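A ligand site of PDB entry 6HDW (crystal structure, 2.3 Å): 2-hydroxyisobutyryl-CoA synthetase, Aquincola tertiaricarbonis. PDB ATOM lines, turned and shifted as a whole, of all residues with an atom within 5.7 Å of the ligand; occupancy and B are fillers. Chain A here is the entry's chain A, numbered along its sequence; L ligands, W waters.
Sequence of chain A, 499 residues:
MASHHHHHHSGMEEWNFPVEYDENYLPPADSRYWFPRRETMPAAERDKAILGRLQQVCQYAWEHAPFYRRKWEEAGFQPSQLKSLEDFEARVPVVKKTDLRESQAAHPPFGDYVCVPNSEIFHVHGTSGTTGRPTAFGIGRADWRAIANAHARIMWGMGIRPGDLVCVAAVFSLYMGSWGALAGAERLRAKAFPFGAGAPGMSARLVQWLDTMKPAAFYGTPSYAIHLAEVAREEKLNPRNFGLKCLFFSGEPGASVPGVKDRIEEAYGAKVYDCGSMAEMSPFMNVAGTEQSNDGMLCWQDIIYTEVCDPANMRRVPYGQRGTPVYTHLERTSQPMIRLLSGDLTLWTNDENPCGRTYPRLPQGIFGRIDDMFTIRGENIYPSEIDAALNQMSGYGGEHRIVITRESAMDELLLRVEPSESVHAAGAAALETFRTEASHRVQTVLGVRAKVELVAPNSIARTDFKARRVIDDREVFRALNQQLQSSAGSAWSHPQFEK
O9 of the ligand is in hydrogen-bond range of OD1 of Asp 344 (2.6 Å).
The side-chain hydroxyl of Tyr 175 sits at hydrogen-bond distance from an oxygen (O1) of the ligand, at 2.7 Å.
OG of Ser 250 sits at hydrogen-bond distance from O1 of the ligand (2.7 Å).
A nitrogen (N5) of the ligand is in hydrogen-bond range of the backbone carbonyl oxygen (O) of Cys 275.
An oxygen (O8) of the ligand lies within hydrogen-bond range of the guanidinium group of Arg 369, at 2.8 Å.
An oxygen (O5) of the ligand sits at hydrogen-bond distance from the backbone NH of Ala 279 (2.9 Å).
An oxygen (O4) of the ligand is in salt-bridge range of the side-chain amino group (NZ) of Lys 466 (3.0 Å).
The backbone NH (N) of Gly 251 sits at hydrogen-bond distance from a nitrogen (N2) of the ligand, at 3.2 Å.
The side-chain carboxylate (OD1) of Asp 274 sits at hydrogen-bond distance from a nitrogen (N5) of the ligand, 3.2 Å away.
O of Gly 276 is in hydrogen-bond range of N5 of the ligand (3.5 Å).
The guanidinium group (NE) of Arg 369 lies within salt-bridge range of the side-chain carboxylate (OD1) of Asp 344, at 3.8 Å.
OG of Ser 342 sits close to N of Asp 344.
OG of Ser 250 lies within hydrogen-bond range of OH of Tyr 219.
The backbone NH (N) of Cys 275 sits close to the side-chain sulfur (SD) of Met 297 (3.8 Å).
The backbone NH (N) of Cys 275 is in hydrogen-bond range of the backbone carbonyl oxygen (O) of Phe 249 (3.0 Å).
The backbone carbonyl oxygen (O) of Ala 279 sits at hydrogen-bond distance from the side-chain hydroxyl (OG) of Ser 282.
The backbone carbonyl oxygen of Phe 284 lies within hydrogen-bond range of the backbone NH of Ser 277 (2.9 Å).
The backbone carbonyl oxygen (O) of Gly 177 sits close to the side-chain hydroxyl (OH) of Tyr 219, at 3.2 Å.
Residues that only touch the ligand: Gly 177, Tyr 219, Glu 252, Pro 253, Ser 277, Met 278, Glu 280, Phe 284 and Ile 366.
Hydrophobic or aromatic side chains within 4 Å of the ligand: Tyr 175, Pro 253, Ala 279, Phe 284 and Ile 366.
The nearest printed residue that does not touch the ligand is Met 297 (4.2 Å).
Water W1 bridges an oxygen (O5) of the ligand (2.7 Å) and the side-chain carboxylate of Glu 280 (2.7 Å).
Water W3 lies within hydrogen-bond range of N4 of the ligand (2.7 Å), OD2 of Asp 274 (2.8 Å) and N of Ile 366 (2.8 Å).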
ATOM      1  N   LYS A  97      23.435  20.569  40.722  1.00  0.00           N
ATOM      2  CA  LYS A  97      24.617  21.120  40.033  1.00  0.00           C
ATOM      3  C   LYS A  97      24.961  22.524  40.585  1.00  0.00           C
ATOM      4  O   LYS A  97      26.134  22.898  40.658  1.00  0.00           O
ATOM      5  CB  LYS A  97      24.388  21.186  38.515  1.00  0.00           C
ATOM      6  CG  LYS A  97      24.818  19.928  37.751  1.00  0.00           C
ATOM      7  CD  LYS A  97      23.643  19.187  37.119  1.00  0.00           C
ATOM      8  CE  LYS A  97      23.190  19.768  35.804  1.00  0.00           C
ATOM      9  NZ  LYS A  97      21.796  19.374  35.494  1.00  0.00           N
ATOM     10  N   THR A 127      33.291  21.704  32.916  1.00  0.00           N
ATOM     11  CA  THR A 127      32.127  22.062  32.102  1.00  0.00           C
ATOM     12  C   THR A 127      32.371  23.413  31.376  1.00  0.00           C
ATOM     13  O   THR A 127      33.296  24.147  31.744  1.00  0.00           O
ATOM     14  CB  THR A 127      30.862  22.150  33.000  1.00  0.00           C
ATOM     15  OG1 THR A 127      31.060  23.154  33.991  1.00  0.00           O
ATOM     16  CG2 THR A 127      30.519  20.835  33.662  1.00  0.00           C
ATOM     17  N   TYR A 175      35.689  18.678  28.302  1.00  0.00           N
ATOM     18  CA  TYR A 175      34.683  17.629  28.041  1.00  0.00           C
ATOM     19  C   TYR A 175      35.168  16.218  28.389  1.00  0.00           C
ATOM     20  O   TYR A 175      36.144  15.743  27.807  1.00  0.00           O
ATOM     21  CB  TYR A 175      34.203  17.691  26.587  1.00  0.00           C
ATOM     22  CG  TYR A 175      33.062  16.746  26.285  1.00  0.00           C
ATOM     23  CD1 TYR A 175      31.880  16.801  27.008  1.00  0.00           C
ATOM     24  CD2 TYR A 175      33.157  15.820  25.246  1.00  0.00           C
ATOM     25  CE1 TYR A 175      30.815  15.943  26.729  1.00  0.00           C
ATOM     26  CE2 TYR A 175      32.083  14.984  24.928  1.00  0.00           C
ATOM     27  CZ  TYR A 175      30.921  15.049  25.674  1.00  0.00           C
ATOM     28  OH  TYR A 175      29.865  14.217  25.411  1.00  0.00           O
ATOM     29  N   MET A 176      34.455  15.553  29.321  1.00  0.00           N
ATOM     30  CA  MET A 176      34.803  14.220  29.837  1.00  0.00           C
ATOM     31  C   MET A 176      34.497  13.050  28.900  1.00  0.00           C
ATOM     32  O   MET A 176      35.081  11.964  29.070  1.00  0.00           O
ATOM     33  CB  MET A 176      34.129  13.963  31.196  1.00  0.00           C
ATOM     34  CG  MET A 176      34.801  14.693  32.365  1.00  0.00           C
ATOM     35  SD  MET A 176      36.477  14.155  32.691  1.00  0.00           S
ATOM     36  CE  MET A 176      36.239  12.511  33.353  1.00  0.00           C
ATOM     37  N   GLY A 177      33.563  13.251  27.968  1.00  0.00           N
ATOM     38  CA  GLY A 177      33.112  12.239  27.027  1.00  0.00           C
ATOM     39  C   GLY A 177      34.217  11.542  26.260  1.00  0.00           C
ATOM     40  O   GLY A 177      34.304  10.312  26.247  1.00  0.00           O
ATOM     41  N   TYR A 219      33.305   6.562  18.449  1.00  0.00           N
ATOM     42  CA  TYR A 219      32.694   7.276  19.568  1.00  0.00           C
ATOM     43  C   TYR A 219      32.580   8.767  19.247  1.00  0.00           C
ATOM     44  O   TYR A 219      33.545   9.368  18.767  1.00  0.00           O
ATOM     45  CB  TYR A 219      33.465   7.073  20.899  1.00  0.00           C
ATOM     46  CG  TYR A 219      32.937   7.966  22.009  1.00  0.00           C
ATOM     47  CD1 TYR A 219      31.830   7.599  22.768  1.00  0.00           C
ATOM     48  CD2 TYR A 219      33.502   9.228  22.237  1.00  0.00           C
ATOM     49  CE1 TYR A 219      31.317   8.450  23.744  1.00  0.00           C
ATOM     50  CE2 TYR A 219      32.979  10.082  23.200  1.00  0.00           C
ATOM     51  CZ  TYR A 219      31.890   9.691  23.953  1.00  0.00           C
ATOM     52  OH  TYR A 219      31.363  10.540  24.888  1.00  0.00           O
ATOM     53  N   PHE A 249      27.508   6.249  21.235  1.00  0.00           N
ATOM     54  CA  PHE A 249      27.395   7.687  21.484  1.00  0.00           C
ATOM     55  C   PHE A 249      26.903   8.047  22.853  1.00  0.00           C
ATOM     56  O   PHE A 249      26.159   7.284  23.479  1.00  0.00           O
ATOM     57  CB  PHE A 249      26.419   8.324  20.463  1.00  0.00           C
ATOM     58  CG  PHE A 249      26.565   7.971  19.004  1.00  0.00           C
ATOM     59  CD1 PHE A 249      27.680   8.380  18.280  1.00  0.00           C
ATOM     60  CD2 PHE A 249      25.547   7.309  18.324  1.00  0.00           C
ATOM     61  CE1 PHE A 249      27.807   8.065  16.926  1.00  0.00           C
ATOM     62  CE2 PHE A 249      25.669   7.004  16.962  1.00  0.00           C
ATOM     63  CZ  PHE A 249      26.788   7.401  16.268  1.00  0.00           C
ATOM     64  N   SER A 250      27.236   9.290  23.261  1.00  0.00           N
ATOM     65  CA  SER A 250      26.773   9.981  24.455  1.00  0.00           C
ATOM     66  C   SER A 250      26.790  11.496  24.203  1.00  0.00           C
ATOM     67  O   SER A 250      27.398  11.969  23.244  1.00  0.00           O
ATOM     68  CB  SER A 250      27.622   9.604  25.667  1.00  0.00           C
ATOM     69  OG  SER A 250      28.865  10.293  25.700  1.00  0.00           O
ATOM     70  N   GLY A 251      26.115  12.250  25.063  1.00  0.00           N
ATOM     71  CA  GLY A 251      26.140  13.701  25.003  1.00  0.00           C
ATOM     72  C   GLY A 251      24.798  14.365  24.853  1.00  0.00           C
ATOM     73  O   GLY A 251      24.623  15.509  25.261  1.00  0.00           O
ATOM     74  N   GLU A 252      23.848  13.639  24.247  1.00  0.00           N
ATOM     75  CA  GLU A 252      22.524  14.149  23.933  1.00  0.00           C
ATOM     76  C   GLU A 252      21.635  12.996  23.461  1.00  0.00           C
ATOM     77  O   GLU A 252      22.180  11.947  23.099  1.00  0.00           O
ATOM     78  CB  GLU A 252      22.645  15.181  22.784  1.00  0.00           C
ATOM     79  CG  GLU A 252      23.462  14.683  21.598  1.00  0.00           C
ATOM     80  CD  GLU A 252      23.427  15.492  20.319  1.00  0.00           C
ATOM     81  OE1 GLU A 252      23.019  16.674  20.350  1.00  0.00           O
ATOM     82  OE2 GLU A 252      23.823  14.924  19.281  1.00  0.00           O
ATOM     83  N   PRO A 253      20.287  13.160  23.376  1.00  0.00           N
ATOM     84  CA  PRO A 253      19.456  12.090  22.813  1.00  0.00           C
ATOM     85  C   PRO A 253      19.732  11.948  21.316  1.00  0.00           C
ATOM     86  O   PRO A 253      20.182  12.902  20.673  1.00  0.00           O
ATOM     87  CB  PRO A 253      18.014  12.570  23.063  1.00  0.00           C
ATOM     88  CG  PRO A 253      18.132  13.721  24.019  1.00  0.00           C
ATOM     89  CD  PRO A 253      19.463  14.338  23.731  1.00  0.00           C
ATOM     90  N   GLY A 254      19.473  10.759  20.783  1.00  0.00           N
ATOM     91  CA  GLY A 254      19.682  10.456  19.370  1.00  0.00           C
ATOM     92  C   GLY A 254      19.827   8.979  19.101  1.00  0.00           C
ATOM     93  O   GLY A 254      19.162   8.449  18.223  1.00  0.00           O
ATOM     94  N   ASP A 274      23.660   3.413  22.534  1.00  0.00           N
ATOM     95  CA  ASP A 274      23.384   4.539  23.413  1.00  0.00           C
ATOM     96  C   ASP A 274      24.093   4.303  24.754  1.00  0.00           C
ATOM     97  O   ASP A 274      24.056   3.187  25.293  1.00  0.00           O
ATOM     98  CB  ASP A 274      21.872   4.672  23.630  1.00  0.00           C
ATOM     99  CG  ASP A 274      21.402   6.001  24.205  1.00  0.00           C
ATOM    100  OD1 ASP A 274      22.116   7.007  24.041  1.00  0.00           O
ATOM    101  OD2 ASP A 274      20.271   6.048  24.732  1.00  0.00           O
ATOM    102  N   CYS A 275      24.762   5.341  25.268  1.00  0.00           N
ATOM    103  CA  CYS A 275      25.421   5.375  26.574  1.00  0.00           C
ATOM    104  C   CYS A 275      25.491   6.815  27.062  1.00  0.00           C
ATOM    105  O   CYS A 275      25.188   7.731  26.295  1.00  0.00           O
ATOM    106  CB  CYS A 275      26.805   4.708  26.550  1.00  0.00           C
ATOM    107  SG  CYS A 275      28.103   5.656  25.725  1.00  0.00           S
ATOM    108  N   GLY A 276      25.861   7.016  28.319  1.00  0.00           N
ATOM    109  CA  GLY A 276      26.058   8.356  28.870  1.00  0.00           C
ATOM    110  C   GLY A 276      25.035   8.887  29.851  1.00  0.00           C
ATOM    111  O   GLY A 276      23.860   9.059  29.524  1.00  0.00           O
ATOM    112  N   SER A 277      25.522   9.214  31.058  1.00  0.00           N
ATOM    113  CA  SER A 277      24.761   9.860  32.127  1.00  0.00           C
ATOM    114  C   SER A 277      25.192  11.336  32.149  1.00  0.00           C
ATOM    115  O   SER A 277      24.717  12.122  31.339  1.00  0.00           O
ATOM    116  CB  SER A 277      24.984   9.168  33.471  1.00  0.00           C
ATOM    117  OG  SER A 277      26.368   9.094  33.789  1.00  0.00           O
ATOM    118  N   MET A 278      26.149  11.706  33.023  1.00  0.00           N
ATOM    119  CA  MET A 278      26.670  13.063  33.191  1.00  0.00           C
ATOM    120  C   MET A 278      28.187  13.007  33.330  1.00  0.00           C
ATOM    121  O   MET A 278      28.713  11.969  33.727  1.00  0.00           O
ATOM    122  CB  MET A 278      26.077  13.692  34.461  1.00  0.00           C
ATOM    123  CG  MET A 278      24.555  13.632  34.554  1.00  0.00           C
ATOM    124  SD  MET A 278      23.969  14.518  36.002  1.00  0.00           S
ATOM    125  CE  MET A 278      23.749  13.306  37.004  1.00  0.00           C
ATOM    126  N   ALA A 279      28.880  14.109  33.043  1.00  0.00           N
ATOM    127  CA  ALA A 279      30.338  14.242  33.187  1.00  0.00           C
ATOM    128  C   ALA A 279      30.719  14.179  34.666  1.00  0.00           C
ATOM    129  O   ALA A 279      31.770  13.637  34.986  1.00  0.00           O
ATOM    130  CB  ALA A 279      30.813  15.549  32.577  1.00  0.00           C
ATOM    131  N   GLU A 280      29.840  14.706  35.565  1.00  0.00           N
ATOM    132  CA  GLU A 280      30.048  14.646  37.020  1.00  0.00           C
ATOM    133  C   GLU A 280      29.984  13.179  37.468  1.00  0.00           C
ATOM    134  O   GLU A 280      30.572  12.825  38.486  1.00  0.00           O
ATOM    135  CB  GLU A 280      28.953  15.424  37.785  1.00  0.00           C
ATOM    136  CG  GLU A 280      28.981  16.933  37.626  1.00  0.00           C
ATOM    137  CD  GLU A 280      28.306  17.513  36.400  1.00  0.00           C
ATOM    138  OE1 GLU A 280      27.804  16.731  35.555  1.00  0.00           O
ATOM    139  OE2 GLU A 280      28.280  18.763  36.268  1.00  0.00           O
ATOM    140  N   SER A 282      31.262  10.477  35.768  1.00  0.00           N
ATOM    141  CA  SER A 282      32.261   9.597  35.154  1.00  0.00           C
ATOM    142  C   SER A 282      32.628   8.523  36.180  1.00  0.00           C
ATOM    143  O   SER A 282      32.839   8.882  37.332  1.00  0.00           O
ATOM    144  CB  SER A 282      33.486  10.381  34.714  1.00  0.00           C
ATOM    145  OG  SER A 282      33.135  11.389  33.778  1.00  0.00           O
ATOM    146  N   PHE A 284      30.698   7.692  33.140  1.00  0.00           N
ATOM    147  CA  PHE A 284      29.395   8.120  32.605  1.00  0.00           C
ATOM    148  C   PHE A 284      28.695   7.052  31.773  1.00  0.00           C
ATOM    149  O   PHE A 284      27.485   7.139  31.555  1.00  0.00           O
ATOM    150  CB  PHE A 284      29.522   9.450  31.829  1.00  0.00           C
ATOM    151  CG  PHE A 284      30.519   9.395  30.692  1.00  0.00           C
ATOM    152  CD1 PHE A 284      30.162   8.875  29.456  1.00  0.00           C
ATOM    153  CD2 PHE A 284      31.828   9.831  30.878  1.00  0.00           C
ATOM    154  CE1 PHE A 284      31.097   8.782  28.431  1.00  0.00           C
ATOM    155  CE2 PHE A 284      32.758   9.748  29.845  1.00  0.00           C
ATOM    156  CZ  PHE A 284      32.392   9.215  28.634  1.00  0.00           C
ATOM    157  N   MET A 297      19.250   1.781  27.040  1.00  0.00           N
ATOM    158  CA  MET A 297      20.430   1.630  27.893  1.00  0.00           C
ATOM    159  C   MET A 297      20.122   0.795  29.125  1.00  0.00           C
ATOM    160  O   MET A 297      19.008   0.850  29.625  1.00  0.00           O
ATOM    161  CB  MET A 297      20.918   3.013  28.367  1.00  0.00           C
ATOM    162  CG  MET A 297      21.409   3.923  27.260  1.00  0.00           C
ATOM    163  SD  MET A 297      22.066   5.496  27.874  1.00  0.00           S
ATOM    164  CE  MET A 297      20.596   6.373  28.209  1.00  0.00           C
ATOM    165  N   SER A 342      20.058  14.667  38.015  1.00  0.00           N
ATOM    166  CA  SER A 342      20.431  14.906  36.613  1.00  0.00           C
ATOM    167  C   SER A 342      19.643  16.035  35.974  1.00  0.00           C
ATOM    168  O   SER A 342      20.213  16.803  35.185  1.00  0.00           O
ATOM    169  CB  SER A 342      20.298  13.629  35.800  1.00  0.00           C
ATOM    170  OG  SER A 342      18.941  13.243  35.693  1.00  0.00           O
ATOM    171  N   ASP A 344      17.146  15.386  34.071  1.00  0.00           N
ATOM    172  CA  ASP A 344      16.744  14.772  32.808  1.00  0.00           C
ATOM    173  C   ASP A 344      15.481  13.981  32.986  1.00  0.00           C
ATOM    174  O   ASP A 344      15.100  13.724  34.130  1.00  0.00           O
ATOM    175  CB  ASP A 344      17.869  13.857  32.289  1.00  0.00           C
ATOM    176  CG  ASP A 344      19.152  14.596  31.986  1.00  0.00           C
ATOM    177  OD1 ASP A 344      19.099  15.613  31.261  1.00  0.00           O
ATOM    178  OD2 ASP A 344      20.208  14.139  32.458  1.00  0.00           O
ATOM    179  N   GLY A 365      15.990   5.296  26.213  1.00  0.00           N
ATOM    180  CA  GLY A 365      17.109   6.122  26.635  1.00  0.00           C
ATOM    181  C   GLY A 365      16.616   7.292  27.462  1.00  0.00           C
ATOM    182  O   GLY A 365      15.689   7.150  28.267  1.00  0.00           O
ATOM    183  N   ILE A 366      17.214   8.464  27.236  1.00  0.00           N
ATOM    184  CA  ILE A 366      16.916   9.701  27.952  1.00  0.00           C
ATOM    185  C   ILE A 366      16.348  10.704  26.951  1.00  0.00           C
ATOM    186  O   ILE A 366      16.948  10.967  25.908  1.00  0.00           O
ATOM    187  CB  ILE A 366      18.158  10.172  28.776  1.00  0.00           C
ATOM    188  CG1 ILE A 366      18.496   9.156  29.891  1.00  0.00           C
ATOM    189  CG2 ILE A 366      17.987  11.604  29.342  1.00  0.00           C
ATOM    190  CD1 ILE A 366      19.941   9.207  30.446  1.00  0.00           C
ATOM    191  N   PHE A 367      15.137  11.223  27.265  1.00  0.00           N
ATOM    192  CA  PHE A 367      14.347  12.107  26.409  1.00  0.00           C
ATOM    193  C   PHE A 367      14.910  13.498  26.257  1.00  0.00           C
ATOM    194  O   PHE A 367      14.721  14.123  25.219  1.00  0.00           O
ATOM    195  CB  PHE A 367      12.886  12.164  26.885  1.00  0.00           C
ATOM    196  CG  PHE A 367      12.263  10.820  27.192  1.00  0.00           C
ATOM    197  CD1 PHE A 367      12.307   9.786  26.268  1.00  0.00           C
ATOM    198  CD2 PHE A 367      11.607  10.609  28.394  1.00  0.00           C
ATOM    199  CE1 PHE A 367      11.724   8.548  26.548  1.00  0.00           C
ATOM    200  CE2 PHE A 367      11.021   9.367  28.683  1.00  0.00           C
ATOM    201  CZ  PHE A 367      11.094   8.339  27.760  1.00  0.00           C
ATOM    202  N   GLY A 368      15.578  13.993  27.294  1.00  0.00           N
ATOM    203  CA  GLY A 368      16.170  15.316  27.317  1.00  0.00           C
ATOM    204  C   GLY A 368      16.183  15.886  28.718  1.00  0.00           C
ATOM    205  O   GLY A 368      15.752  15.216  29.662  1.00  0.00           O
ATOM    206  N   ARG A 369      16.665  17.124  28.848  1.00  0.00           N
ATOM    207  CA  ARG A 369      16.732  17.857  30.115  1.00  0.00           C
ATOM    208  C   ARG A 369      15.366  18.523  30.333  1.00  0.00           C
ATOM    209  O   ARG A 369      14.825  19.123  29.408  1.00  0.00           O
ATOM    210  CB  ARG A 369      17.868  18.892  30.051  1.00  0.00           C
ATOM    211  CG  ARG A 369      18.326  19.410  31.403  1.00  0.00           C
ATOM    212  CD  ARG A 369      19.781  19.850  31.360  1.00  0.00           C
ATOM    213  NE  ARG A 369      20.644  18.985  32.157  1.00  0.00           N
ATOM    214  CZ  ARG A 369      21.961  18.921  32.025  1.00  0.00           C
ATOM    215  NH1 ARG A 369      22.588  19.654  31.110  1.00  0.00           N
ATOM    216  NH2 ARG A 369      22.672  18.104  32.794  1.00  0.00           N
ATOM    217  N   PHE A 465      29.708  18.342  18.115  1.00  0.00           N
ATOM    218  CA  PHE A 465      29.369  18.283  19.536  1.00  0.00           C
ATOM    219  C   PHE A 465      27.843  18.097  19.682  1.00  0.00           C
ATOM    220  O   PHE A 465      27.256  17.330  18.922  1.00  0.00           O
ATOM    221  CB  PHE A 465      29.945  19.506  20.287  1.00  0.00           C
ATOM    222  CG  PHE A 465      29.966  19.409  21.802  1.00  0.00           C
ATOM    223  CD1 PHE A 465      30.607  18.351  22.438  1.00  0.00           C
ATOM    224  CD2 PHE A 465      29.370  20.391  22.593  1.00  0.00           C
ATOM    225  CE1 PHE A 465      30.635  18.251  23.835  1.00  0.00           C
ATOM    226  CE2 PHE A 465      29.398  20.291  23.990  1.00  0.00           C
ATOM    227  CZ  PHE A 465      30.035  19.227  24.599  1.00  0.00           C
ATOM    228  N   LYS A 466      27.213  18.773  20.659  1.00  0.00           N
ATOM    229  CA  LYS A 466      25.795  18.676  20.968  1.00  0.00           C
ATOM    230  C   LYS A 466      24.975  19.684  20.152  1.00  0.00           C
ATOM    231  O   LYS A 466      25.285  20.879  20.143  1.00  0.00           O
ATOM    232  CB  LYS A 466      25.554  18.931  22.476  1.00  0.00           C
ATOM    233  CG  LYS A 466      26.330  18.010  23.414  1.00  0.00           C
ATOM    234  CD  LYS A 466      26.157  18.444  24.870  1.00  0.00           C
ATOM    235  CE  LYS A 466      26.980  17.620  25.826  1.00  0.00           C
ATOM    236  NZ  LYS A 466      26.680  17.951  27.234  1.00  0.00           N
HETATM  237  C1  LIG L   1      20.198  11.631  26.345  1.00  0.00           C
HETATM  238  C2  LIG L   1      30.066  12.876  29.310  1.00  0.00           C
HETATM  239  C3  LIG L   1      28.685  12.867  28.635  1.00  0.00           C
HETATM  240  C4  LIG L   1      27.791  11.784  29.273  1.00  0.00           C
HETATM  241  O1  LIG L   1      28.842  12.525  27.267  1.00  0.00           O
HETATM  242  C5  LIG L   1      28.034  14.272  28.731  1.00  0.00           C
HETATM  243  O2  LIG L   1      27.670  14.862  27.721  1.00  0.00           O
HETATM  244  O3  LIG L   1      27.928  14.787  29.994  1.00  0.00           O
HETATM  245  P1  LIG L   1      27.597  16.345  30.380  1.00  0.00           P
HETATM  246  O4  LIG L   1      28.504  17.305  29.487  1.00  0.00           O
HETATM  247  O5  LIG L   1      27.764  16.549  31.837  1.00  0.00           O
HETATM  248  O6  LIG L   1      26.090  16.575  29.981  1.00  0.00           O
HETATM  249  C6  LIG L   1      25.158  15.664  30.527  1.00  0.00           C
HETATM  250  C7  LIG L   1      23.796  15.929  29.937  1.00  0.00           C
HETATM  251  O7  LIG L   1      23.839  15.586  28.529  1.00  0.00           O
HETATM  252  C8  LIG L   1      22.873  14.959  30.551  1.00  0.00           C
HETATM  253  O8  LIG L   1      22.333  15.529  31.751  1.00  0.00           O
HETATM  254  C9  LIG L   1      21.826  14.795  29.457  1.00  0.00           C
HETATM  255  O9  LIG L   1      20.893  15.907  29.391  1.00  0.00           O
HETATM  256  C10 LIG L   1      22.680  14.786  28.211  1.00  0.00           C
HETATM  257  N1  LIG L   1      23.062  13.399  27.800  1.00  0.00           N
HETATM  258  C11 LIG L   1      24.247  12.777  27.916  1.00  0.00           C
HETATM  259  N2  LIG L   1      24.129  11.558  27.417  1.00  0.00           N
HETATM  260  C12 LIG L   1      22.863  11.392  27.007  1.00  0.00           C
HETATM  261  C13 LIG L   1      22.203  12.544  27.253  1.00  0.00           C
HETATM  262  N3  LIG L   1      20.898  12.691  26.916  1.00  0.00           N
HETATM  263  N4  LIG L   1      20.912  10.451  26.103  1.00  0.00           N
HETATM  264  C14 LIG L   1      22.215  10.369  26.414  1.00  0.00           C
HETATM  265  N5  LIG L   1      22.894   9.259  26.172  1.00  0.00           N
HETATM  266  O   HOH W   1      26.048  17.625  33.661  1.00  0.00           O
HETATM  267  O   HOH W   2      30.648  18.690  30.445  1.00  0.00           O
HETATM  268  O   HOH W   3      19.147   8.584  25.185  1.00  0.00           O
HETATM  269  O   HOH W   4      19.290  15.249  27.262  1.00  0.00           O
HETATM  270  O   HOH W   5      22.245  11.554  30.385  1.00  0.00           O
